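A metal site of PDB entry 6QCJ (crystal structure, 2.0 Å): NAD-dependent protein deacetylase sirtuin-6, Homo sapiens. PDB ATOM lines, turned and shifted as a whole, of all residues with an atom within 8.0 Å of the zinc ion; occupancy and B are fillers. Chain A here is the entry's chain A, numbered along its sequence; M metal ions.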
ATOM      1  N   GLU A 134      25.691   4.683  -8.903  1.00  0.00           N
ATOM      2  CA  GLU A 134      25.149   5.942  -8.357  1.00  0.00           C
ATOM      3  C   GLU A 134      24.716   5.722  -6.915  1.00  0.00           C
ATOM      4  O   GLU A 134      23.896   4.847  -6.684  1.00  0.00           O
ATOM      5  CB  GLU A 134      23.940   6.373  -9.184  1.00  0.00           C
ATOM      6  CG  GLU A 134      23.183   7.567  -8.618  1.00  0.00           C
ATOM      7  CD  GLU A 134      22.241   8.145  -9.665  1.00  0.00           C
ATOM      8  OE1 GLU A 134      22.687   8.466 -10.734  1.00  0.00           O
ATOM      9  OE2 GLU A 134      21.045   8.253  -9.406  1.00  0.00           O
ATOM     10  N   CYS A 135      25.166   6.597  -6.018  1.00  0.00           N
ATOM     11  CA  CYS A 135      24.689   6.665  -4.618  1.00  0.00           C
ATOM     12  C   CYS A 135      23.168   6.868  -4.602  1.00  0.00           C
ATOM     13  O   CYS A 135      22.686   7.873  -5.140  1.00  0.00           O
ATOM     14  CB  CYS A 135      25.336   7.811  -3.853  1.00  0.00           C
ATOM     15  SG  CYS A 135      25.169   7.611  -2.057  1.00  0.00           S
ATOM     16  N   ALA A 136      22.455   5.950  -3.965  1.00  0.00           N
ATOM     17  CA  ALA A 136      21.058   6.160  -3.542  1.00  0.00           C
ATOM     18  C   ALA A 136      20.952   7.464  -2.734  1.00  0.00           C
ATOM     19  O   ALA A 136      19.958   8.179  -2.915  1.00  0.00           O
ATOM     20  CB  ALA A 136      20.599   4.970  -2.726  1.00  0.00           C
ATOM     21  N   LYS A 137      21.939   7.787  -1.891  1.00  0.00           N
ATOM     22  CA  LYS A 137      21.788   8.831  -0.822  1.00  0.00           C
ATOM     23  C   LYS A 137      22.086  10.238  -1.352  1.00  0.00           C
ATOM     24  O   LYS A 137      21.298  11.142  -1.009  1.00  0.00           O
ATOM     25  CB  LYS A 137      22.653   8.530   0.403  1.00  0.00           C
ATOM     26  CG  LYS A 137      22.077   7.437   1.295  1.00  0.00           C
ATOM     27  CD  LYS A 137      22.382   7.592   2.765  1.00  0.00           C
ATOM     28  CE  LYS A 137      21.940   6.365   3.545  1.00  0.00           C
ATOM     29  NZ  LYS A 137      21.450   6.703   4.907  1.00  0.00           N
ATOM     30  N   CYS A 138      23.163  10.419  -2.128  1.00  0.00           N
ATOM     31  CA  CYS A 138      23.725  11.760  -2.491  1.00  0.00           C
ATOM     32  C   CYS A 138      23.689  11.987  -4.010  1.00  0.00           C
ATOM     33  O   CYS A 138      23.960  13.125  -4.450  1.00  0.00           O
ATOM     34  CB  CYS A 138      25.107  11.950  -1.868  1.00  0.00           C
ATOM     35  SG  CYS A 138      26.454  10.913  -2.522  1.00  0.00           S
ATOM     36  N   LYS A 139      23.387  10.944  -4.792  1.00  0.00           N
ATOM     37  CA  LYS A 139      23.227  10.992  -6.255  1.00  0.00           C
ATOM     38  C   LYS A 139      24.611  10.963  -6.922  1.00  0.00           C
ATOM     39  O   LYS A 139      24.696  11.268  -8.123  1.00  0.00           O
ATOM     40  CB  LYS A 139      22.459  12.254  -6.664  1.00  0.00           C
ATOM     41  N   THR A 140      25.656  10.628  -6.184  1.00  0.00           N
ATOM     42  CA  THR A 140      27.028  10.729  -6.755  1.00  0.00           C
ATOM     43  C   THR A 140      27.327   9.480  -7.600  1.00  0.00           C
ATOM     44  O   THR A 140      27.064   8.357  -7.125  1.00  0.00           O
ATOM     45  CB  THR A 140      28.032  11.083  -5.675  1.00  0.00           C
ATOM     46  OG1 THR A 140      27.457  12.211  -5.011  1.00  0.00           O
ATOM     47  CG2 THR A 140      29.421  11.380  -6.176  1.00  0.00           C
ATOM     48  N   GLN A 141      27.736   9.725  -8.854  1.00  0.00           N
ATOM     49  CA  GLN A 141      27.999   8.708  -9.908  1.00  0.00           C
ATOM     50  C   GLN A 141      29.495   8.393  -9.964  1.00  0.00           C
ATOM     51  O   GLN A 141      30.301   9.308  -9.805  1.00  0.00           O
ATOM     52  CB  GLN A 141      27.565   9.215 -11.288  1.00  0.00           C
ATOM     53  CG  GLN A 141      26.078   9.495 -11.343  1.00  0.00           C
ATOM     54  CD  GLN A 141      25.582   9.698 -12.742  1.00  0.00           C
ATOM     55  OE1 GLN A 141      26.224  10.306 -13.591  1.00  0.00           O
ATOM     56  NE2 GLN A 141      24.392   9.173 -12.985  1.00  0.00           N
ATOM     57  N   TYR A 142      29.841   7.126 -10.118  1.00  0.00           N
ATOM     58  CA  TYR A 142      31.248   6.669 -10.098  1.00  0.00           C
ATOM     59  C   TYR A 142      31.509   5.934 -11.401  1.00  0.00           C
ATOM     60  O   TYR A 142      30.758   5.021 -11.634  1.00  0.00           O
ATOM     61  CB  TYR A 142      31.545   5.682  -8.954  1.00  0.00           C
ATOM     62  CG  TYR A 142      31.455   6.212  -7.542  1.00  0.00           C
ATOM     63  CD1 TYR A 142      30.247   6.570  -6.964  1.00  0.00           C
ATOM     64  CD2 TYR A 142      32.595   6.260  -6.734  1.00  0.00           C
ATOM     65  CE1 TYR A 142      30.175   7.039  -5.661  1.00  0.00           C
ATOM     66  CE2 TYR A 142      32.537   6.726  -5.430  1.00  0.00           C
ATOM     67  CZ  TYR A 142      31.316   7.120  -4.891  1.00  0.00           C
ATOM     68  OH  TYR A 142      31.242   7.570  -3.610  1.00  0.00           O
ATOM     69  N   LEU A 159      29.536   0.762  -1.285  1.00  0.00           N
ATOM     70  CA  LEU A 159      28.972   1.855  -0.459  1.00  0.00           C
ATOM     71  C   LEU A 159      29.692   3.153  -0.826  1.00  0.00           C
ATOM     72  O   LEU A 159      30.897   3.094  -1.195  1.00  0.00           O
ATOM     73  CB  LEU A 159      29.142   1.519   1.021  1.00  0.00           C
ATOM     74  CG  LEU A 159      28.627   0.152   1.459  1.00  0.00           C
ATOM     75  CD1 LEU A 159      29.272  -0.300   2.761  1.00  0.00           C
ATOM     76  CD2 LEU A 159      27.114   0.169   1.591  1.00  0.00           C
ATOM     77  N   CYS A 160      28.993   4.279  -0.744  1.00  0.00           N
ATOM     78  CA  CYS A 160      29.567   5.600  -1.110  1.00  0.00           C
ATOM     79  C   CYS A 160      30.736   5.930  -0.193  1.00  0.00           C
ATOM     80  O   CYS A 160      30.658   5.582   1.008  1.00  0.00           O
ATOM     81  CB  CYS A 160      28.546   6.703  -0.930  1.00  0.00           C
ATOM     82  SG  CYS A 160      28.898   8.212  -1.847  1.00  0.00           S
ATOM     83  N   THR A 161      31.717   6.651  -0.747  1.00  0.00           N
ATOM     84  CA  THR A 161      32.997   7.033  -0.123  1.00  0.00           C
ATOM     85  C   THR A 161      33.168   8.544  -0.223  1.00  0.00           C
ATOM     86  O   THR A 161      34.308   9.013  -0.040  1.00  0.00           O
ATOM     87  CB  THR A 161      34.174   6.309  -0.811  1.00  0.00           C
ATOM     88  OG1 THR A 161      34.314   6.820  -2.133  1.00  0.00           O
ATOM     89  CG2 THR A 161      34.001   4.809  -0.957  1.00  0.00           C
ATOM     90  N   VAL A 162      32.105   9.310  -0.518  1.00  0.00           N
ATOM     91  CA  VAL A 162      32.187  10.800  -0.439  1.00  0.00           C
ATOM     92  C   VAL A 162      32.155  11.201   1.043  1.00  0.00           C
ATOM     93  O   VAL A 162      31.397  10.581   1.771  1.00  0.00           O
ATOM     94  CB  VAL A 162      31.055  11.518  -1.186  1.00  0.00           C
ATOM     95  CG1 VAL A 162      31.148  13.034  -0.999  1.00  0.00           C
ATOM     96  CG2 VAL A 162      31.014  11.153  -2.664  1.00  0.00           C
ATOM     97  N   ALA A 163      32.901  12.233   1.436  1.00  0.00           N
ATOM     98  CA  ALA A 163      32.612  13.024   2.673  1.00  0.00           C
ATOM     99  C   ALA A 163      32.687  14.519   2.360  1.00  0.00           C
ATOM    100  O   ALA A 163      33.645  15.143   2.876  1.00  0.00           O
ATOM    101  CB  ALA A 163      33.534  12.639   3.806  1.00  0.00           C
ATOM    102  N   CYS A 171      29.521   9.436   3.959  1.00  0.00           N
ATOM    103  CA  CYS A 171      28.161   9.221   3.375  1.00  0.00           C
ATOM    104  C   CYS A 171      27.771   7.764   3.551  1.00  0.00           C
ATOM    105  O   CYS A 171      26.749   7.467   4.169  1.00  0.00           O
ATOM    106  CB  CYS A 171      28.133   9.583   1.887  1.00  0.00           C
ATOM    107  SG  CYS A 171      26.729   8.861   1.017  1.00  0.00           S
ATOM    108  N   ARG A 172      28.556   6.862   2.951  1.00  0.00           N
ATOM    109  CA  ARG A 172      28.356   5.406   3.090  1.00  0.00           C
ATOM    110  C   ARG A 172      26.988   5.002   2.522  1.00  0.00           C
ATOM    111  O   ARG A 172      26.563   3.902   2.811  1.00  0.00           O
ATOM    112  CB  ARG A 172      28.493   5.004   4.564  1.00  0.00           C
ATOM    113  CG  ARG A 172      29.745   5.536   5.257  1.00  0.00           C
ATOM    114  CD  ARG A 172      29.911   4.857   6.615  1.00  0.00           C
ATOM    115  NE  ARG A 172      29.854   3.394   6.557  1.00  0.00           N
ATOM    116  CZ  ARG A 172      30.858   2.602   6.201  1.00  0.00           C
ATOM    117  NH1 ARG A 172      32.039   3.092   5.871  1.00  0.00           N
ATOM    118  NH2 ARG A 172      30.690   1.294   6.178  1.00  0.00           N
ATOM    119  N   GLY A 173      26.357   5.822   1.677  1.00  0.00           N
ATOM    120  CA  GLY A 173      25.075   5.450   1.017  1.00  0.00           C
ATOM    121  C   GLY A 173      25.175   4.176   0.165  1.00  0.00           C
ATOM    122  O   GLY A 173      26.304   3.664  -0.120  1.00  0.00           O
ATOM    123  N   GLU A 174      24.032   3.670  -0.287  1.00  0.00           N
ATOM    124  CA  GLU A 174      23.971   2.434  -1.110  1.00  0.00           C
ATOM    125  C   GLU A 174      24.317   2.804  -2.563  1.00  0.00           C
ATOM    126  O   GLU A 174      23.674   3.726  -3.070  1.00  0.00           O
ATOM    127  CB  GLU A 174      22.589   1.796  -0.971  1.00  0.00           C
ATOM    128  CG  GLU A 174      22.480   0.395  -1.550  1.00  0.00           C
ATOM    129  CD  GLU A 174      21.173  -0.304  -1.213  1.00  0.00           C
ATOM    130  OE1 GLU A 174      20.572  -0.910  -2.126  1.00  0.00           O
ATOM    131  OE2 GLU A 174      20.771  -0.234  -0.048  1.00  0.00           O
ATOM    132  N   LEU A 175      25.293   2.110  -3.183  1.00  0.00           N
ATOM    133  CA  LEU A 175      25.579   2.231  -4.638  1.00  0.00           C
ATOM    134  C   LEU A 175      24.713   1.231  -5.378  1.00  0.00           C
ATOM    135  O   LEU A 175      24.651   0.042  -4.967  1.00  0.00           O
ATOM    136  CB  LEU A 175      27.062   2.010  -4.974  1.00  0.00           C
ATOM    137  CG  LEU A 175      28.111   2.965  -4.370  1.00  0.00           C
ATOM    138  CD1 LEU A 175      29.362   2.922  -5.239  1.00  0.00           C
ATOM    139  CD2 LEU A 175      27.653   4.412  -4.215  1.00  0.00           C
HETATM  140 ZN    ZN M   1      26.758   9.068  -1.264  1.00  0.00          ZN
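The side-chain sulfur of Cys 138 lies close to the side-chain hydroxyl of Thr 140, 3.0 Å away. N of Cys 171 is in hydrogen-bond range of O of Val 162 (3.1 Å). The backbone NH (N) of Gly 173 sits close to the side-chain sulfur (SG) of Cys 171, at 3.1 Å. The side-chain sulfur (SG) of Cys 160 lies close to the side-chain hydroxyl (OH) of Tyr 142, at 3.0 Å. The backbone NH (N) of Cys 135 lies within hydrogen-bond range of the backbone carbonyl oxygen (O) of Thr 140 (2.8 Å). The backbone carbonyl oxygen (O) of Cys 160 sits close to the backbone NH (N) of Arg 172 (3.1 Å). The backbone NH (N) of Lys 137 lies close to the side-chain sulfur (SG) of Cys 135 (3.2 Å). The side-chain sulfur of Cys 160 sits close to the backbone NH of Val 162.
Four residues have an atom within 4 Å of the zinc ion: Cys 135, Cys 138, Cys 160 and Cys 171.
The side-chain sulfur (SG) of Cys 138 is bound to the zinc ion, at 2.3 Å. The side-chain sulfur (SG) of Cys 171 binds the zinc ion. The side-chain sulfur (SG) of Cys 135 is bound to the zinc ion, at 2.3 Å. The zinc ion is bound by the side-chain sulfur (SG) of Cys 160 (2.4 Å).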
